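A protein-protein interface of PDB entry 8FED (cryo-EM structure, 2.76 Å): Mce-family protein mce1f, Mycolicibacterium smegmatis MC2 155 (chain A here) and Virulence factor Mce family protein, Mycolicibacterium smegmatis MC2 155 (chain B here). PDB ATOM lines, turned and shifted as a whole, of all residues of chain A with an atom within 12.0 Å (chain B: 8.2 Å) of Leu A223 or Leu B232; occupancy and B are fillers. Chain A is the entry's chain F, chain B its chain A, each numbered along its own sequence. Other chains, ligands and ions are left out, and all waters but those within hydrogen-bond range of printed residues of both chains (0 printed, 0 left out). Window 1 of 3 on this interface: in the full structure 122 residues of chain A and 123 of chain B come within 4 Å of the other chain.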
ATOM      1  N   GLN A 209     -23.598 -24.198 -23.213  1.00  0.00           N
ATOM      2  CA  GLN A 209     -22.699 -23.255 -22.556  1.00  0.00           C
ATOM      3  C   GLN A 209     -21.703 -22.645 -23.537  1.00  0.00           C
ATOM      4  O   GLN A 209     -21.328 -21.477 -23.389  1.00  0.00           O
ATOM      5  CB  GLN A 209     -21.970 -23.938 -21.401  1.00  0.00           C
ATOM      6  CG  GLN A 209     -22.869 -24.306 -20.231  1.00  0.00           C
ATOM      7  CD  GLN A 209     -23.497 -23.098 -19.557  1.00  0.00           C
ATOM      8  OE1 GLN A 209     -22.998 -21.978 -19.665  1.00  0.00           O
ATOM      9  NE2 GLN A 209     -24.601 -23.323 -18.856  1.00  0.00           N
ATOM     10  N   GLY A 213     -21.076 -18.159 -25.067  1.00  0.00           N
ATOM     11  CA  GLY A 213     -19.835 -17.705 -24.455  1.00  0.00           C
ATOM     12  C   GLY A 213     -19.785 -16.203 -24.243  1.00  0.00           C
ATOM     13  O   GLY A 213     -19.305 -15.727 -23.209  1.00  0.00           O
ATOM     14  N   ASP A 214     -20.266 -15.436 -25.223  1.00  0.00           N
ATOM     15  CA  ASP A 214     -20.247 -13.984 -25.095  1.00  0.00           C
ATOM     16  C   ASP A 214     -21.096 -13.526 -23.918  1.00  0.00           C
ATOM     17  O   ASP A 214     -20.699 -12.627 -23.170  1.00  0.00           O
ATOM     18  CB  ASP A 214     -20.728 -13.336 -26.392  1.00  0.00           C
ATOM     19  CG  ASP A 214     -19.908 -13.762 -27.593  1.00  0.00           C
ATOM     20  OD1 ASP A 214     -18.717 -14.089 -27.412  1.00  0.00           O
ATOM     21  OD2 ASP A 214     -20.452 -13.769 -28.716  1.00  0.00           O
ATOM     22  N   ALA A 215     -22.265 -14.145 -23.732  1.00  0.00           N
ATOM     23  CA  ALA A 215     -23.143 -13.759 -22.633  1.00  0.00           C
ATOM     24  C   ALA A 215     -22.511 -14.047 -21.278  1.00  0.00           C
ATOM     25  O   ALA A 215     -22.597 -13.221 -20.360  1.00  0.00           O
ATOM     26  CB  ALA A 215     -24.487 -14.473 -22.759  1.00  0.00           C
ATOM     27  N   ILE A 216     -21.881 -15.216 -21.121  1.00  0.00           N
ATOM     28  CA  ILE A 216     -21.299 -15.542 -19.821  1.00  0.00           C
ATOM     29  C   ILE A 216     -20.087 -14.664 -19.542  1.00  0.00           C
ATOM     30  O   ILE A 216     -19.892 -14.211 -18.408  1.00  0.00           O
ATOM     31  CB  ILE A 216     -20.980 -17.044 -19.689  1.00  0.00           C
ATOM     32  CG1 ILE A 216     -20.212 -17.582 -20.888  1.00  0.00           C
ATOM     33  CG2 ILE A 216     -22.255 -17.838 -19.466  1.00  0.00           C
ATOM     34  CD1 ILE A 216     -20.085 -19.090 -20.882  1.00  0.00           C
ATOM     35  N   GLN A 217     -19.271 -14.385 -20.563  1.00  0.00           N
ATOM     36  CA  GLN A 217     -18.168 -13.446 -20.372  1.00  0.00           C
ATOM     37  C   GLN A 217     -18.676 -12.060 -19.982  1.00  0.00           C
ATOM     38  O   GLN A 217     -18.122 -11.416 -19.079  1.00  0.00           O
ATOM     39  CB  GLN A 217     -17.316 -13.364 -21.638  1.00  0.00           C
ATOM     40  CG  GLN A 217     -16.538 -14.628 -21.949  1.00  0.00           C
ATOM     41  CD  GLN A 217     -15.693 -14.493 -23.199  1.00  0.00           C
ATOM     42  OE1 GLN A 217     -15.579 -13.409 -23.769  1.00  0.00           O
ATOM     43  NE2 GLN A 217     -15.097 -15.597 -23.632  1.00  0.00           N
ATOM     44  N   ARG A 218     -19.736 -11.590 -20.645  1.00  0.00           N
ATOM     45  CA  ARG A 218     -20.273 -10.264 -20.358  1.00  0.00           C
ATOM     46  C   ARG A 218     -20.832 -10.171 -18.944  1.00  0.00           C
ATOM     47  O   ARG A 218     -20.560  -9.202 -18.224  1.00  0.00           O
ATOM     48  CB  ARG A 218     -21.347  -9.908 -21.386  1.00  0.00           C
ATOM     49  CG  ARG A 218     -22.002  -8.558 -21.157  1.00  0.00           C
ATOM     50  CD  ARG A 218     -20.990  -7.429 -21.226  1.00  0.00           C
ATOM     51  NE  ARG A 218     -21.597  -6.137 -20.937  1.00  0.00           N
ATOM     52  CZ  ARG A 218     -20.934  -4.989 -20.899  1.00  0.00           C
ATOM     53  NH1 ARG A 218     -19.632  -4.936 -21.127  1.00  0.00           N
ATOM     54  NH2 ARG A 218     -21.593  -3.868 -20.623  1.00  0.00           N
ATOM     55  N   TRP A 219     -21.613 -11.169 -18.512  1.00  0.00           N
ATOM     56  CA  TRP A 219     -22.136 -11.070 -17.153  1.00  0.00           C
ATOM     57  C   TRP A 219     -21.070 -11.352 -16.106  1.00  0.00           C
ATOM     58  O   TRP A 219     -21.189 -10.848 -14.989  1.00  0.00           O
ATOM     59  CB  TRP A 219     -23.371 -11.962 -16.933  1.00  0.00           C
ATOM     60  CG  TRP A 219     -23.158 -13.433 -16.684  1.00  0.00           C
ATOM     61  CD1 TRP A 219     -23.369 -14.435 -17.571  1.00  0.00           C
ATOM     62  CD2 TRP A 219     -22.759 -14.066 -15.455  1.00  0.00           C
ATOM     63  NE1 TRP A 219     -23.093 -15.651 -16.998  1.00  0.00           N
ATOM     64  CE2 TRP A 219     -22.717 -15.452 -15.697  1.00  0.00           C
ATOM     65  CE3 TRP A 219     -22.420 -13.595 -14.182  1.00  0.00           C
ATOM     66  CZ2 TRP A 219     -22.351 -16.370 -14.717  1.00  0.00           C
ATOM     67  CZ3 TRP A 219     -22.052 -14.508 -13.213  1.00  0.00           C
ATOM     68  CH2 TRP A 219     -22.023 -15.880 -13.485  1.00  0.00           C
ATOM     69  N   ALA A 220     -20.011 -12.094 -16.441  1.00  0.00           N
ATOM     70  CA  ALA A 220     -18.889 -12.216 -15.516  1.00  0.00           C
ATOM     71  C   ALA A 220     -18.205 -10.870 -15.311  1.00  0.00           C
ATOM     72  O   ALA A 220     -17.912 -10.474 -14.174  1.00  0.00           O
ATOM     73  CB  ALA A 220     -17.896 -13.255 -16.033  1.00  0.00           C
ATOM     74  N   ALA A 221     -17.950 -10.145 -16.404  1.00  0.00           N
ATOM     75  CA  ALA A 221     -17.341  -8.823 -16.287  1.00  0.00           C
ATOM     76  C   ALA A 221     -18.246  -7.857 -15.527  1.00  0.00           C
ATOM     77  O   ALA A 221     -17.774  -7.071 -14.693  1.00  0.00           O
ATOM     78  CB  ALA A 221     -17.011  -8.272 -17.673  1.00  0.00           C
ATOM     79  N   ASN A 222     -19.550  -7.898 -15.804  1.00  0.00           N
ATOM     80  CA  ASN A 222     -20.479  -7.015 -15.106  1.00  0.00           C
ATOM     81  C   ASN A 222     -20.595  -7.370 -13.627  1.00  0.00           C
ATOM     82  O   ASN A 222     -20.745  -6.478 -12.784  1.00  0.00           O
ATOM     83  CB  ASN A 222     -21.844  -7.054 -15.781  1.00  0.00           C
ATOM     84  CG  ASN A 222     -21.801  -6.537 -17.199  1.00  0.00           C
ATOM     85  OD1 ASN A 222     -20.731  -6.279 -17.748  1.00  0.00           O
ATOM     86  ND2 ASN A 222     -22.969  -6.381 -17.804  1.00  0.00           N
ATOM     87  N   LEU A 223     -20.551  -8.662 -13.293  1.00  0.00           N
ATOM     88  CA  LEU A 223     -20.516  -9.064 -11.892  1.00  0.00           C
ATOM     89  C   LEU A 223     -19.257  -8.547 -11.217  1.00  0.00           C
ATOM     90  O   LEU A 223     -19.307  -8.082 -10.074  1.00  0.00           O
ATOM     91  CB  LEU A 223     -20.599 -10.585 -11.774  1.00  0.00           C
ATOM     92  CG  LEU A 223     -20.362 -11.154 -10.374  1.00  0.00           C
ATOM     93  CD1 LEU A 223     -21.465 -10.721  -9.419  1.00  0.00           C
ATOM     94  CD2 LEU A 223     -20.237 -12.668 -10.413  1.00  0.00           C
ATOM     95  N   ASN A 224     -18.118  -8.629 -11.911  1.00  0.00           N
ATOM     96  CA  ASN A 224     -16.876  -8.074 -11.383  1.00  0.00           C
ATOM     97  C   ASN A 224     -17.036  -6.591 -11.069  1.00  0.00           C
ATOM     98  O   ASN A 224     -16.687  -6.133  -9.975  1.00  0.00           O
ATOM     99  CB  ASN A 224     -15.745  -8.296 -12.389  1.00  0.00           C
ATOM    100  CG  ASN A 224     -14.434  -7.680 -11.945  1.00  0.00           C
ATOM    101  OD1 ASN A 224     -14.172  -7.536 -10.752  1.00  0.00           O
ATOM    102  ND2 ASN A 224     -13.601  -7.314 -12.911  1.00  0.00           N
ATOM    103  N   THR A 225     -17.588  -5.832 -12.020  1.00  0.00           N
ATOM    104  CA  THR A 225     -17.744  -4.391 -11.838  1.00  0.00           C
ATOM    105  C   THR A 225     -18.692  -4.072 -10.684  1.00  0.00           C
ATOM    106  O   THR A 225     -18.379  -3.245  -9.816  1.00  0.00           O
ATOM    107  CB  THR A 225     -18.244  -3.756 -13.135  1.00  0.00           C
ATOM    108  OG1 THR A 225     -17.258  -3.923 -14.160  1.00  0.00           O
ATOM    109  CG2 THR A 225     -18.512  -2.277 -12.935  1.00  0.00           C
ATOM    110  N   LEU A 226     -19.863  -4.716 -10.662  1.00  0.00           N
ATOM    111  CA  LEU A 226     -20.842  -4.454  -9.611  1.00  0.00           C
ATOM    112  C   LEU A 226     -20.302  -4.835  -8.242  1.00  0.00           C
ATOM    113  O   LEU A 226     -20.502  -4.107  -7.262  1.00  0.00           O
ATOM    114  CB  LEU A 226     -22.141  -5.208  -9.893  1.00  0.00           C
ATOM    115  CG  LEU A 226     -23.045  -4.674 -11.002  1.00  0.00           C
ATOM    116  CD1 LEU A 226     -24.233  -5.595 -11.206  1.00  0.00           C
ATOM    117  CD2 LEU A 226     -23.512  -3.267 -10.672  1.00  0.00           C
ATOM    118  N   ALA A 227     -19.620  -5.979  -8.150  1.00  0.00           N
ATOM    119  CA  ALA A 227     -19.058  -6.409  -6.879  1.00  0.00           C
ATOM    120  C   ALA A 227     -17.970  -5.458  -6.407  1.00  0.00           C
ATOM    121  O   ALA A 227     -17.889  -5.149  -5.214  1.00  0.00           O
ATOM    122  CB  ALA A 227     -18.522  -7.833  -7.005  1.00  0.00           C
ATOM    123  N   ALA A 228     -17.122  -4.982  -7.325  1.00  0.00           N
ATOM    124  CA  ALA A 228     -16.095  -4.015  -6.952  1.00  0.00           C
ATOM    125  C   ALA A 228     -16.720  -2.734  -6.418  1.00  0.00           C
ATOM    126  O   ALA A 228     -16.294  -2.202  -5.385  1.00  0.00           O
ATOM    127  CB  ALA A 228     -15.192  -3.719  -8.150  1.00  0.00           C
ATOM    128  N   GLN A 229     -17.749  -2.231  -7.107  1.00  0.00           N
ATOM    129  CA  GLN A 229     -18.414  -1.012  -6.653  1.00  0.00           C
ATOM    130  C   GLN A 229     -19.074  -1.214  -5.294  1.00  0.00           C
ATOM    131  O   GLN A 229     -19.046  -0.316  -4.444  1.00  0.00           O
ATOM    132  CB  GLN A 229     -19.443  -0.553  -7.686  1.00  0.00           C
ATOM    133  CG  GLN A 229     -18.842  -0.130  -9.013  1.00  0.00           C
ATOM    134  CD  GLN A 229     -19.890   0.347  -9.994  1.00  0.00           C
ATOM    135  OE1 GLN A 229     -21.030   0.614  -9.622  1.00  0.00           O
ATOM    136  NE2 GLN A 229     -19.509   0.452 -11.259  1.00  0.00           N
ATOM    137  N   SER A 230     -19.680  -2.383  -5.073  1.00  0.00           N
ATOM    138  CA  SER A 230     -20.339  -2.643  -3.798  1.00  0.00           C
ATOM    139  C   SER A 230     -19.335  -2.817  -2.666  1.00  0.00           C
ATOM    140  O   SER A 230     -19.618  -2.433  -1.525  1.00  0.00           O
ATOM    141  CB  SER A 230     -21.228  -3.881  -3.908  1.00  0.00           C
ATOM    142  OG  SER A 230     -20.471  -5.015  -4.287  1.00  0.00           O
ATOM    143  N   ALA A 231     -18.168  -3.396  -2.954  1.00  0.00           N
ATOM    144  CA  ALA A 231     -17.163  -3.603  -1.918  1.00  0.00           C
ATOM    145  C   ALA A 231     -16.427  -2.319  -1.567  1.00  0.00           C
ATOM    146  O   ALA A 231     -16.065  -2.120  -0.403  1.00  0.00           O
ATOM    147  CB  ALA A 231     -16.163  -4.672  -2.359  1.00  0.00           C
ATOM    148  N   GLN A 232     -16.198  -1.440  -2.546  1.00  0.00           N
ATOM    149  CA  GLN A 232     -15.506  -0.186  -2.270  1.00  0.00           C
ATOM    150  C   GLN A 232     -16.320   0.762  -1.399  1.00  0.00           C
ATOM    151  O   GLN A 232     -15.763   1.745  -0.898  1.00  0.00           O
ATOM    152  CB  GLN A 232     -15.133   0.508  -3.581  1.00  0.00           C
ATOM    153  CG  GLN A 232     -14.022  -0.182  -4.352  1.00  0.00           C
ATOM    154  CD  GLN A 232     -13.814   0.416  -5.728  1.00  0.00           C
ATOM    155  OE1 GLN A 232     -14.533   1.328  -6.135  1.00  0.00           O
ATOM    156  NE2 GLN A 232     -12.829  -0.097  -6.454  1.00  0.00           N
ATOM    157  N   TYR B 225     -14.413 -20.509 -20.399  1.00  0.00           N
ATOM    158  CA  TYR B 225     -14.289 -20.360 -18.954  1.00  0.00           C
ATOM    159  C   TYR B 225     -12.940 -19.769 -18.567  1.00  0.00           C
ATOM    160  O   TYR B 225     -12.856 -18.985 -17.618  1.00  0.00           O
ATOM    161  CB  TYR B 225     -14.504 -21.708 -18.267  1.00  0.00           C
ATOM    162  CG  TYR B 225     -15.957 -22.056 -18.032  1.00  0.00           C
ATOM    163  CD1 TYR B 225     -16.955 -21.109 -18.211  1.00  0.00           C
ATOM    164  CD2 TYR B 225     -16.327 -23.327 -17.618  1.00  0.00           C
ATOM    165  CE1 TYR B 225     -18.283 -21.421 -17.992  1.00  0.00           C
ATOM    166  CE2 TYR B 225     -17.653 -23.649 -17.395  1.00  0.00           C
ATOM    167  CZ  TYR B 225     -18.625 -22.691 -17.583  1.00  0.00           C
ATOM    168  OH  TYR B 225     -19.946 -23.005 -17.365  1.00  0.00           O
ATOM    169  N   ASP B 227     -11.258 -17.662 -20.414  1.00  0.00           N
ATOM    170  CA  ASP B 227     -11.364 -16.243 -20.742  1.00  0.00           C
ATOM    171  C   ASP B 227     -12.158 -15.480 -19.685  1.00  0.00           C
ATOM    172  O   ASP B 227     -11.807 -14.346 -19.339  1.00  0.00           O
ATOM    173  CB  ASP B 227     -11.999 -16.068 -22.120  1.00  0.00           C
ATOM    174  CG  ASP B 227     -11.080 -16.501 -23.242  1.00  0.00           C
ATOM    175  OD1 ASP B 227      -9.931 -16.892 -22.951  1.00  0.00           O
ATOM    176  OD2 ASP B 227     -11.505 -16.448 -24.415  1.00  0.00           O
ATOM    177  N   ALA B 228     -13.230 -16.076 -19.168  1.00  0.00           N
ATOM    178  CA  ALA B 228     -14.132 -15.374 -18.261  1.00  0.00           C
ATOM    179  C   ALA B 228     -13.795 -15.552 -16.784  1.00  0.00           C
ATOM    180  O   ALA B 228     -14.445 -14.924 -15.943  1.00  0.00           O
ATOM    181  CB  ALA B 228     -15.576 -15.827 -18.501  1.00  0.00           C
ATOM    182  N   SER B 229     -12.815 -16.398 -16.446  1.00  0.00           N
ATOM    183  CA  SER B 229     -12.557 -16.704 -15.038  1.00  0.00           C
ATOM    184  C   SER B 229     -12.041 -15.527 -14.212  1.00  0.00           C
ATOM    185  O   SER B 229     -12.561 -15.325 -13.101  1.00  0.00           O
ATOM    186  CB  SER B 229     -11.622 -17.915 -14.940  1.00  0.00           C
ATOM    187  OG  SER B 229     -10.668 -17.925 -15.984  1.00  0.00           O
ATOM    188  N   PRO B 230     -11.021 -14.755 -14.636  1.00  0.00           N
ATOM    189  CA  PRO B 230     -10.488 -13.718 -13.727  1.00  0.00           C
ATOM    190  C   PRO B 230     -11.525 -12.711 -13.258  1.00  0.00           C
ATOM    191  O   PRO B 230     -11.543 -12.347 -12.072  1.00  0.00           O
ATOM    192  CB  PRO B 230      -9.393 -13.048 -14.568  1.00  0.00           C
ATOM    193  CG  PRO B 230      -8.993 -14.073 -15.548  1.00  0.00           C
ATOM    194  CD  PRO B 230     -10.252 -14.790 -15.896  1.00  0.00           C
ATOM    195  N   ASP B 231     -12.403 -12.267 -14.159  1.00  0.00           N
ATOM    196  CA  ASP B 231     -13.457 -11.339 -13.770  1.00  0.00           C
ATOM    197  C   ASP B 231     -14.396 -11.987 -12.763  1.00  0.00           C
ATOM    198  O   ASP B 231     -14.791 -11.357 -11.773  1.00  0.00           O
ATOM    199  CB  ASP B 231     -14.228 -10.876 -15.005  1.00  0.00           C
ATOM    200  CG  ASP B 231     -13.329 -10.650 -16.203  1.00  0.00           C
ATOM    201  OD1 ASP B 231     -12.112 -10.905 -16.092  1.00  0.00           O
ATOM    202  OD2 ASP B 231     -13.839 -10.220 -17.259  1.00  0.00           O
ATOM    203  N   LEU B 232     -14.751 -13.253 -12.996  1.00  0.00           N
ATOM    204  CA  LEU B 232     -15.635 -13.961 -12.079  1.00  0.00           C
ATOM    205  C   LEU B 232     -15.015 -14.073 -10.694  1.00  0.00           C
ATOM    206  O   LEU B 232     -15.700 -13.884  -9.686  1.00  0.00           O
ATOM    207  CB  LEU B 232     -15.961 -15.350 -12.625  1.00  0.00           C
ATOM    208  CG  LEU B 232     -16.731 -16.245 -11.651  1.00  0.00           C
ATOM    209  CD1 LEU B 232     -18.145 -15.728 -11.444  1.00  0.00           C
ATOM    210  CD2 LEU B 232     -16.739 -17.691 -12.112  1.00  0.00           C
ATOM    211  N   PHE B 233     -13.713 -14.354 -10.621  1.00  0.00           N
ATOM    212  CA  PHE B 233     -13.095 -14.554  -9.315  1.00  0.00           C
ATOM    213  C   PHE B 233     -12.892 -13.235  -8.576  1.00  0.00           C
ATOM    214  O   PHE B 233     -13.032 -13.185  -7.348  1.00  0.00           O
ATOM    215  CB  PHE B 233     -11.775 -15.310  -9.466  1.00  0.00           C
ATOM    216  CG  PHE B 233     -11.953 -16.774  -9.750  1.00  0.00           C
ATOM    217  CD1 PHE B 233     -12.488 -17.616  -8.791  1.00  0.00           C
ATOM    218  CD2 PHE B 233     -11.582 -17.309 -10.970  1.00  0.00           C
ATOM    219  CE1 PHE B 233     -12.656 -18.960  -9.046  1.00  0.00           C
ATOM    220  CE2 PHE B 233     -11.747 -18.656 -11.231  1.00  0.00           C
ATOM    221  CZ  PHE B 233     -12.283 -19.481 -10.267  1.00  0.00           C
ATOM    222  N   ASP B 234     -12.569 -12.155  -9.297  1.00  0.00           N
ATOM    223  CA  ASP B 234     -12.518 -10.845  -8.651  1.00  0.00           C
ATOM    224  C   ASP B 234     -13.889 -10.450  -8.114  1.00  0.00           C
ATOM    225  O   ASP B 234     -14.014  -9.963  -6.976  1.00  0.00           O
ATOM    226  CB  ASP B 234     -11.998  -9.794  -9.631  1.00  0.00           C
ATOM    227  CG  ASP B 234     -10.621 -10.130 -10.170  1.00  0.00           C
ATOM    228  OD1 ASP B 234     -10.102 -11.217  -9.842  1.00  0.00           O
ATOM    229  OD2 ASP B 234     -10.057  -9.308 -10.921  1.00  0.00           O
ATOM    230  N   GLY B 235     -14.933 -10.660  -8.922  1.00  0.00           N
ATOM    231  CA  GLY B 235     -16.281 -10.416  -8.455  1.00  0.00           C
ATOM    232  C   GLY B 235     -16.658 -11.282  -7.274  1.00  0.00           C
ATOM    233  O   GLY B 235     -17.378 -10.838  -6.386  1.00  0.00           O
ATOM    234  N   LEU B 236     -16.166 -12.522  -7.239  1.00  0.00           N
ATOM    235  CA  LEU B 236     -16.442 -13.398  -6.105  1.00  0.00           C
ATOM    236  C   LEU B 236     -15.745 -12.912  -4.841  1.00  0.00           C
ATOM    237  O   LEU B 236     -16.309 -13.004  -3.749  1.00  0.00           O
ATOM    238  CB  LEU B 236     -16.030 -14.833  -6.429  1.00  0.00           C
ATOM    239  CG  LEU B 236     -16.990 -15.632  -7.313  1.00  0.00           C
ATOM    240  CD1 LEU B 236     -16.483 -17.051  -7.505  1.00  0.00           C
ATOM    241  CD2 LEU B 236     -18.390 -15.633  -6.720  1.00  0.00           C
ATOM    242  N   ASP B 237     -14.520 -12.396  -4.964  1.00  0.00           N
ATOM    243  CA  ASP B 237     -13.838 -11.817  -3.807  1.00  0.00           C
ATOM    244  C   ASP B 237     -14.625 -10.644  -3.234  1.00  0.00           C
ATOM    245  O   ASP B 237     -14.917 -10.588  -2.028  1.00  0.00           O
ATOM    246  CB  ASP B 237     -12.431 -11.365  -4.201  1.00  0.00           C
ATOM    247  CG  ASP B 237     -11.447 -12.507  -4.259  1.00  0.00           C
ATOM    248  OD1 ASP B 237     -11.401 -13.300  -3.296  1.00  0.00           O
ATOM    249  OD2 ASP B 237     -10.720 -12.617  -5.269  1.00  0.00           O
ATOM    250  N   ASN B 238     -14.985  -9.692  -4.096  1.00  0.00           N
ATOM    251  CA  ASN B 238     -15.734  -8.536  -3.613  1.00  0.00           C
ATOM    252  C   ASN B 238     -17.131  -8.931  -3.138  1.00  0.00           C
ATOM    253  O   ASN B 238     -17.677  -8.314  -2.209  1.00  0.00           O
ATOM    254  CB  ASN B 238     -15.790  -7.473  -4.704  1.00  0.00           C
ATOM    255  CG  ASN B 238     -14.415  -6.948  -5.070  1.00  0.00           C
ATOM    256  OD1 ASN B 238     -13.572  -6.730  -4.201  1.00  0.00           O
ATOM    257  ND2 ASN B 238     -14.178  -6.752  -6.361  1.00  0.00           N
ATOM    258  N   ALA B 239     -17.713  -9.968  -3.741  1.00  0.00           N
ATOM    259  CA  ALA B 239     -18.999 -10.475  -3.294  1.00  0.00           C
ATOM    260  C   ALA B 239     -18.887 -11.144  -1.935  1.00  0.00           C
ATOM    261  O   ALA B 239     -19.832 -11.092  -1.150  1.00  0.00           O
ATOM    262  CB  ALA B 239     -19.567 -11.446  -4.326  1.00  0.00           C
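Gln A209 touches Tyr B225 (OE1 to OH, 3.96 Å).
Gln A217 touches Ala B228 (CG to CB, 3.8 Å).
Ala A220 touches Ala B228 (CB to O, 3.8 Å).
Ala A220 touches Asp B231.
Asp B231 touches Ala A221.
Asn A224 touches Asp B231.
Asn A224 touches Gly B235 (OD1 to N, 3.7 Å).
CB of Ala A227 touches O of Gly B235 (3.3 Å).
Ala A227 touches Asn B238 (O to CB, 3.2 Å).
Ala A228 touches Asn B238 (CA to ND2, 3.4 Å).
The side-chain hydroxyl (OG1) of Thr A225 is in hydrogen-bond range of the backbone carbonyl oxygen (O) of Ala A221 (3.2 Å).
The side-chain hydroxyl (OG) of Ser A230 lies within hydrogen-bond range of the backbone carbonyl oxygen (O) of Ala A227 (2.7 Å).
The backbone carbonyl oxygen (O) of Tyr B225 is in hydrogen-bond range of the side-chain hydroxyl (OG) of Ser B229 (2.9 Å).
The backbone carbonyl oxygen (O) of Asp B234 sits at hydrogen-bond distance from the side-chain amide nitrogen (ND2) of Asn B238, at 3.3 Å.
Leu A223 touches one residue of chain B.
Of chain A, only Leu A223 (3.8 Å) comes within 4 Å of Leu B232.
Printed residues of chain A within 4 Å of Ala B228: Gln A217 (3.8 Å) and Ala A220 (3.8 Å).
No residue of chain A comes within 4 Å of Ser B229.
Of the printed residues of chain A, Asp B231 touches Ala A220 (3.8 Å), Ala A221 (3.7 Å) and Asn A224 (3.3 Å).
No residue of chain A comes within 4 Å of Phe B233.
Of the printed residues of chain A, Gly B235 touches Asn A224 (3.7 Å) and Ala A227 (3.3 Å).
No residue of chain A comes within 4 Å of Leu B236.
Printed residues of chain B within 4 Å of Gln A217: Asp B227 and Ala B228.
Of the printed residues of chain A, Tyr B225 touches Gln A209 (3.96 Å).
Printed residues of chain B within 4 Å of Ala A221: Asp B231 (3.7 Å).
The nearest printed residue of chain A that does not touch Tyr B225 is Ile A216 (4.1 Å).
Printed residues of chain B that touch a printed residue of chain A: Tyr B225, Asp B227, Ala B228, Asp B231, Leu B232, Asp B234, Gly B235, Asn B238 and Ala B239.
Among the printed residues, no Asp or Glu carboxylate lies within 4 Å of a Lys or Arg side-chain nitrogen of the other chain.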
